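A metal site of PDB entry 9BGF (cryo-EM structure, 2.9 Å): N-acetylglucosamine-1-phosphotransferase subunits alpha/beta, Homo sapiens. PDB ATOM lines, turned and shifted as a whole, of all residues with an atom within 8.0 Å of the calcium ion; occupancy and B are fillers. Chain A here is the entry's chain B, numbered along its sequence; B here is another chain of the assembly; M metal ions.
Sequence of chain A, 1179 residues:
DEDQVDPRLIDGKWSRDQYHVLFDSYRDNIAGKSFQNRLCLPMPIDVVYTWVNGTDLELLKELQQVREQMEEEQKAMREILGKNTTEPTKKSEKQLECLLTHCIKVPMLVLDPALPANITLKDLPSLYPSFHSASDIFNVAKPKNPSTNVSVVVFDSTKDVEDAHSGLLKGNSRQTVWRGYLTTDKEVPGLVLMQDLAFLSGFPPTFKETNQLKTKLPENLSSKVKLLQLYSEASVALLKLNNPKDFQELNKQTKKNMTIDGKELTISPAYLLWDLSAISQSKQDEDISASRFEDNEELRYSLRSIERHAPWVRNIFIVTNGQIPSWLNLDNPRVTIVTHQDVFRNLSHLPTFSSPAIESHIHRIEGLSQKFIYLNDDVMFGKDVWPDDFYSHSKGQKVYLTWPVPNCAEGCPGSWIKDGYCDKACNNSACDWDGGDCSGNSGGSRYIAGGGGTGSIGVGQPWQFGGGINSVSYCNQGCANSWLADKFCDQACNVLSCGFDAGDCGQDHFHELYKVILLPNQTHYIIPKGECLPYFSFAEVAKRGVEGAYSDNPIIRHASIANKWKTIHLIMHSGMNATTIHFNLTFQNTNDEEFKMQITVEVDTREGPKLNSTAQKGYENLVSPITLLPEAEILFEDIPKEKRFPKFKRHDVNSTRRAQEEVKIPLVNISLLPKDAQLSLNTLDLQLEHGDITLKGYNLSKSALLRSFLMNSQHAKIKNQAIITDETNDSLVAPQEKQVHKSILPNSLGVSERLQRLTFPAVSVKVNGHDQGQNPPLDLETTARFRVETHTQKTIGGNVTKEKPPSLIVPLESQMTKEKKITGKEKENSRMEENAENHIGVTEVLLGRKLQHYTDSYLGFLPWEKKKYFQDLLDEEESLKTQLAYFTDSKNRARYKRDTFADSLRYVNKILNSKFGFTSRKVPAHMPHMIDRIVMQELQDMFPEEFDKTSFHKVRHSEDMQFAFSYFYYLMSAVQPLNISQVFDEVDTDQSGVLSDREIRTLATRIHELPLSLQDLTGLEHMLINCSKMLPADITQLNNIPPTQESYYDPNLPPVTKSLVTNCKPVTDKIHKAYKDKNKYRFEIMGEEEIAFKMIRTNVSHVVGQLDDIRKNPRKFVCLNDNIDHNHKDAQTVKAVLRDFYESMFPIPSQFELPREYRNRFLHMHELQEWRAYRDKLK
The side-chain carboxylate (OE1) of Glu 999 sits close to the backbone NH (N) of Ser 996 (2.9 Å). The backbone NH (N) of Gly 993 is in hydrogen-bond range of the side-chain carboxylate (OD2) of Asp 988, 3.1 Å away. NE2 of Gln 991 is in hydrogen-bond range of O of Asp 988, 3.4 Å away.
OG of Ser 996 touches the calcium ion, at 3.9 Å. Six residues have an atom within 4 Å of the calcium ion: Asp 988, Asp 990, Ser 992, Val 994, Ser 996 and Glu 999.
OD1 of Asp 990 is bound to the calcium ion. OG of Ser 992 binds the calcium ion (2.3 Å). The calcium ion is bound by the backbone carbonyl oxygen (O) of Val 994 (2.3 Å). OD1 of Asp 988 is bound to the calcium ion (2.4 Å). The calcium ion is bound by OD2 of Asp 990 (2.5 Å). The calcium ion is bound by OE1 of Glu 999 (2.5 Å). Slightly farther from the calcium ion lies OE2 of Glu 999 (2.9 Å).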
ATOM      1  N   PHE A 984      22.245   6.835  34.874  1.00  0.00           N
ATOM      2  CA  PHE A 984      21.723   6.589  33.534  1.00  0.00           C
ATOM      3  C   PHE A 984      20.427   5.804  33.582  1.00  0.00           C
ATOM      4  O   PHE A 984      19.473   6.122  32.862  1.00  0.00           O
ATOM      5  CB  PHE A 984      22.765   5.845  32.697  1.00  0.00           C
ATOM      6  CG  PHE A 984      22.356   5.638  31.269  1.00  0.00           C
ATOM      7  CD1 PHE A 984      22.567   6.635  30.319  1.00  0.00           C
ATOM      8  CD2 PHE A 984      21.741   4.463  30.867  1.00  0.00           C
ATOM      9  CE1 PHE A 984      22.186   6.451  29.013  1.00  0.00           C
ATOM     10  CE2 PHE A 984      21.360   4.279  29.560  1.00  0.00           C
ATOM     11  CZ  PHE A 984      21.571   5.272  28.633  1.00  0.00           C
ATOM     12  N   VAL A 987      17.604   8.009  34.648  1.00  0.00           N
ATOM     13  CA  VAL A 987      17.225   8.979  33.627  1.00  0.00           C
ATOM     14  C   VAL A 987      16.602   8.285  32.417  1.00  0.00           C
ATOM     15  O   VAL A 987      15.602   8.761  31.877  1.00  0.00           O
ATOM     16  CB  VAL A 987      18.435   9.842  33.229  1.00  0.00           C
ATOM     17  CG1 VAL A 987      18.123  10.643  31.990  1.00  0.00           C
ATOM     18  CG2 VAL A 987      18.798  10.767  34.377  1.00  0.00           C
ATOM     19  N   ASP A 988      17.175   7.168  31.982  1.00  0.00           N
ATOM     20  CA  ASP A 988      16.623   6.389  30.871  1.00  0.00           C
ATOM     21  C   ASP A 988      15.426   5.618  31.398  1.00  0.00           C
ATOM     22  O   ASP A 988      15.531   4.459  31.815  1.00  0.00           O
ATOM     23  CB  ASP A 988      17.682   5.468  30.290  1.00  0.00           C
ATOM     24  CG  ASP A 988      17.131   4.568  29.196  1.00  0.00           C
ATOM     25  OD1 ASP A 988      16.802   5.090  28.115  1.00  0.00           O
ATOM     26  OD2 ASP A 988      17.052   3.344  29.424  1.00  0.00           O
ATOM     27  N   THR A 989      14.259   6.259  31.378  1.00  0.00           N
ATOM     28  CA  THR A 989      13.064   5.694  32.021  1.00  0.00           C
ATOM     29  C   THR A 989      12.343   4.664  31.162  1.00  0.00           C
ATOM     30  O   THR A 989      11.490   3.955  31.683  1.00  0.00           O
ATOM     31  CB  THR A 989      12.086   6.816  32.385  1.00  0.00           C
ATOM     32  OG1 THR A 989      11.832   7.634  31.241  1.00  0.00           O
ATOM     33  CG2 THR A 989      12.657   7.675  33.492  1.00  0.00           C
ATOM     34  N   ASP A 990      12.664   4.563  29.869  1.00  0.00           N
ATOM     35  CA  ASP A 990      11.986   3.619  28.983  1.00  0.00           C
ATOM     36  C   ASP A 990      12.722   2.295  28.865  1.00  0.00           C
ATOM     37  O   ASP A 990      12.296   1.452  28.066  1.00  0.00           O
ATOM     38  CB  ASP A 990      11.803   4.238  27.598  1.00  0.00           C
ATOM     39  CG  ASP A 990      13.117   4.691  26.987  1.00  0.00           C
ATOM     40  OD1 ASP A 990      14.100   4.807  27.747  1.00  0.00           O
ATOM     41  OD2 ASP A 990      13.155   4.925  25.771  1.00  0.00           O
ATOM     42  N   GLN A 991      13.797   2.089  29.622  1.00  0.00           N
ATOM     43  CA  GLN A 991      14.565   0.843  29.607  1.00  0.00           C
ATOM     44  C   GLN A 991      15.044   0.488  28.210  1.00  0.00           C
ATOM     45  O   GLN A 991      15.009  -0.662  27.780  1.00  0.00           O
ATOM     46  CB  GLN A 991      13.743  -0.308  30.196  1.00  0.00           C
ATOM     47  CG  GLN A 991      13.861  -0.463  31.712  1.00  0.00           C
ATOM     48  CD  GLN A 991      13.491   0.799  32.458  1.00  0.00           C
ATOM     49  OE1 GLN A 991      12.323   1.181  32.513  1.00  0.00           O
ATOM     50  NE2 GLN A 991      14.494   1.455  33.030  1.00  0.00           N
ATOM     51  N   SER A 992      15.499   1.503  27.474  1.00  0.00           N
ATOM     52  CA  SER A 992      15.981   1.314  26.108  1.00  0.00           C
ATOM     53  C   SER A 992      17.503   1.320  26.001  1.00  0.00           C
ATOM     54  O   SER A 992      18.037   0.789  25.029  1.00  0.00           O
ATOM     55  CB  SER A 992      15.418   2.397  25.191  1.00  0.00           C
ATOM     56  OG  SER A 992      15.822   3.687  25.606  1.00  0.00           O
ATOM     57  N   GLY A 993      18.197   1.899  26.976  1.00  0.00           N
ATOM     58  CA  GLY A 993      19.624   2.051  26.906  1.00  0.00           C
ATOM     59  C   GLY A 993      20.110   3.280  26.169  1.00  0.00           C
ATOM     60  O   GLY A 993      21.315   3.524  26.145  1.00  0.00           O
ATOM     61  N   VAL A 994      19.207   4.044  25.564  1.00  0.00           N
ATOM     62  CA  VAL A 994      19.560   5.248  24.813  1.00  0.00           C
ATOM     63  C   VAL A 994      18.723   6.410  25.344  1.00  0.00           C
ATOM     64  O   VAL A 994      17.515   6.255  25.551  1.00  0.00           O
ATOM     65  CB  VAL A 994      19.347   5.071  23.301  1.00  0.00           C
ATOM     66  CG1 VAL A 994      19.889   6.272  22.550  1.00  0.00           C
ATOM     67  CG2 VAL A 994      19.984   3.791  22.803  1.00  0.00           C
ATOM     68  N   LEU A 995      19.366   7.541  25.567  1.00  0.00           N
ATOM     69  CA  LEU A 995      18.664   8.729  26.053  1.00  0.00           C
ATOM     70  C   LEU A 995      17.996   9.449  24.889  1.00  0.00           C
ATOM     71  O   LEU A 995      18.668   9.873  23.953  1.00  0.00           O
ATOM     72  CB  LEU A 995      19.637   9.659  26.779  1.00  0.00           C
ATOM     73  CG  LEU A 995      20.220   9.178  28.100  1.00  0.00           C
ATOM     74  CD1 LEU A 995      20.960  10.314  28.799  1.00  0.00           C
ATOM     75  CD2 LEU A 995      19.148   8.601  29.004  1.00  0.00           C
ATOM     76  N   SER A 996      16.679   9.600  24.974  1.00  0.00           N
ATOM     77  CA  SER A 996      15.930  10.372  23.995  1.00  0.00           C
ATOM     78  C   SER A 996      16.029  11.860  24.323  1.00  0.00           C
ATOM     79  O   SER A 996      16.710  12.267  25.269  1.00  0.00           O
ATOM     80  CB  SER A 996      14.487   9.901  23.953  1.00  0.00           C
ATOM     81  OG  SER A 996      14.410   8.502  23.749  1.00  0.00           O
ATOM     82  N   ASP A 997      15.350  12.685  23.525  1.00  0.00           N
ATOM     83  CA  ASP A 997      15.414  14.128  23.750  1.00  0.00           C
ATOM     84  C   ASP A 997      14.842  14.509  25.119  1.00  0.00           C
ATOM     85  O   ASP A 997      15.400  15.366  25.813  1.00  0.00           O
ATOM     86  CB  ASP A 997      14.666  14.867  22.644  1.00  0.00           C
ATOM     87  CG  ASP A 997      15.551  15.192  21.465  1.00  0.00           C
ATOM     88  OD1 ASP A 997      16.787  14.996  21.568  1.00  0.00           O
ATOM     89  OD2 ASP A 997      15.018  15.651  20.427  1.00  0.00           O
ATOM     90  N   ARG A 998      13.735  13.879  25.511  1.00  0.00           N
ATOM     91  CA  ARG A 998      13.157  14.164  26.828  1.00  0.00           C
ATOM     92  C   ARG A 998      14.063  13.688  27.948  1.00  0.00           C
ATOM     93  O   ARG A 998      14.222  14.385  28.966  1.00  0.00           O
ATOM     94  CB  ARG A 998      11.779  13.507  26.924  1.00  0.00           C
ATOM     95  CG  ARG A 998      11.728  12.092  26.378  1.00  0.00           C
ATOM     96  CD  ARG A 998      10.326  11.534  26.449  1.00  0.00           C
ATOM     97  NE  ARG A 998       9.381  12.303  25.645  1.00  0.00           N
ATOM     98  CZ  ARG A 998       8.836  11.889  24.526  1.00  0.00           C
ATOM     99  NH1 ARG A 998       9.101  10.687  24.026  1.00  0.00           N
ATOM    100  NH2 ARG A 998       7.992  12.684  23.868  1.00  0.00           N
ATOM    101  N   GLU A 999      14.663  12.514  27.794  1.00  0.00           N
ATOM    102  CA  GLU A 999      15.582  12.009  28.805  1.00  0.00           C
ATOM    103  C   GLU A 999      16.851  12.849  28.870  1.00  0.00           C
ATOM    104  O   GLU A 999      17.382  13.103  29.953  1.00  0.00           O
ATOM    105  CB  GLU A 999      15.895  10.539  28.528  1.00  0.00           C
ATOM    106  CG  GLU A 999      14.690   9.651  28.741  1.00  0.00           C
ATOM    107  CD  GLU A 999      14.756   8.349  27.978  1.00  0.00           C
ATOM    108  OE1 GLU A 999      15.769   8.104  27.300  1.00  0.00           O
ATOM    109  OE2 GLU A 999      13.786   7.573  28.056  1.00  0.00           O
ATOM    110  N   ILE A1000      17.348  13.307  27.716  1.00  0.00           N
ATOM    111  CA  ILE A1000      18.467  14.242  27.723  1.00  0.00           C
ATOM    112  C   ILE A1000      18.083  15.537  28.428  1.00  0.00           C
ATOM    113  O   ILE A1000      18.887  16.142  29.150  1.00  0.00           O
ATOM    114  CB  ILE A1000      18.966  14.498  26.291  1.00  0.00           C
ATOM    115  CG1 ILE A1000      19.634  13.250  25.731  1.00  0.00           C
ATOM    116  CG2 ILE A1000      19.922  15.681  26.252  1.00  0.00           C
ATOM    117  CD1 ILE A1000      19.966  13.357  24.259  1.00  0.00           C
ATOM    118  N   GLU A1046      14.886   5.693  17.006  1.00  0.00           N
ATOM    119  CA  GLU A1046      14.720   6.984  17.662  1.00  0.00           C
ATOM    120  C   GLU A1046      15.152   8.123  16.747  1.00  0.00           C
ATOM    121  O   GLU A1046      15.682   7.882  15.655  1.00  0.00           O
ATOM    122  CB  GLU A1046      15.535   7.026  18.966  1.00  0.00           C
ATOM    123  CG  GLU A1046      17.039   7.118  18.769  1.00  0.00           C
ATOM    124  CD  GLU A1046      17.689   5.782  18.444  1.00  0.00           C
ATOM    125  OE1 GLU A1046      17.134   5.020  17.630  1.00  0.00           O
ATOM    126  OE2 GLU A1046      18.767   5.500  19.012  1.00  0.00           O
ATOM    127  N   TYR A1048      16.489  12.545  16.946  1.00  0.00           N
ATOM    128  CA  TYR A1048      16.894  13.699  17.733  1.00  0.00           C
ATOM    129  C   TYR A1048      16.630  14.984  16.960  1.00  0.00           C
ATOM    130  O   TYR A1048      16.687  14.998  15.729  1.00  0.00           O
ATOM    131  CB  TYR A1048      18.375  13.624  18.129  1.00  0.00           C
ATOM    132  CG  TYR A1048      18.722  12.487  19.063  1.00  0.00           C
ATOM    133  CD1 TYR A1048      18.470  12.574  20.422  1.00  0.00           C
ATOM    134  CD2 TYR A1048      19.303  11.332  18.577  1.00  0.00           C
ATOM    135  CE1 TYR A1048      18.784  11.548  21.270  1.00  0.00           C
ATOM    136  CE2 TYR A1048      19.623  10.282  19.426  1.00  0.00           C
ATOM    137  CZ  TYR A1048      19.364  10.405  20.777  1.00  0.00           C
ATOM    138  OH  TYR A1048      19.675   9.370  21.623  1.00  0.00           O
ATOM    139  N   VAL A1056      22.674   8.406  22.331  1.00  0.00           N
ATOM    140  CA  VAL A1056      23.301   8.589  23.634  1.00  0.00           C
ATOM    141  C   VAL A1056      23.105   7.336  24.478  1.00  0.00           C
ATOM    142  O   VAL A1056      22.110   7.203  25.193  1.00  0.00           O
ATOM    143  CB  VAL A1056      22.717   9.825  24.347  1.00  0.00           C
ATOM    144  CG1 VAL A1056      23.509  10.142  25.592  1.00  0.00           C
ATOM    145  CG2 VAL A1056      22.699  11.009  23.409  1.00  0.00           C
ATOM    146  N   PRO B1147       7.217   6.439  30.166  1.00  0.00           N
ATOM    147  CA  PRO B1147       7.082   6.091  28.744  1.00  0.00           C
ATOM    148  C   PRO B1147       6.390   4.762  28.524  1.00  0.00           C
ATOM    149  O   PRO B1147       5.661   4.595  27.531  1.00  0.00           O
ATOM    150  CB  PRO B1147       8.534   6.035  28.254  1.00  0.00           C
ATOM    151  CG  PRO B1147       9.395   6.493  29.409  1.00  0.00           C
ATOM    152  CD  PRO B1147       8.599   6.257  30.644  1.00  0.00           C
HETATM  153 CA    CA M   1      15.375   5.824  26.359  1.00  0.00          CA
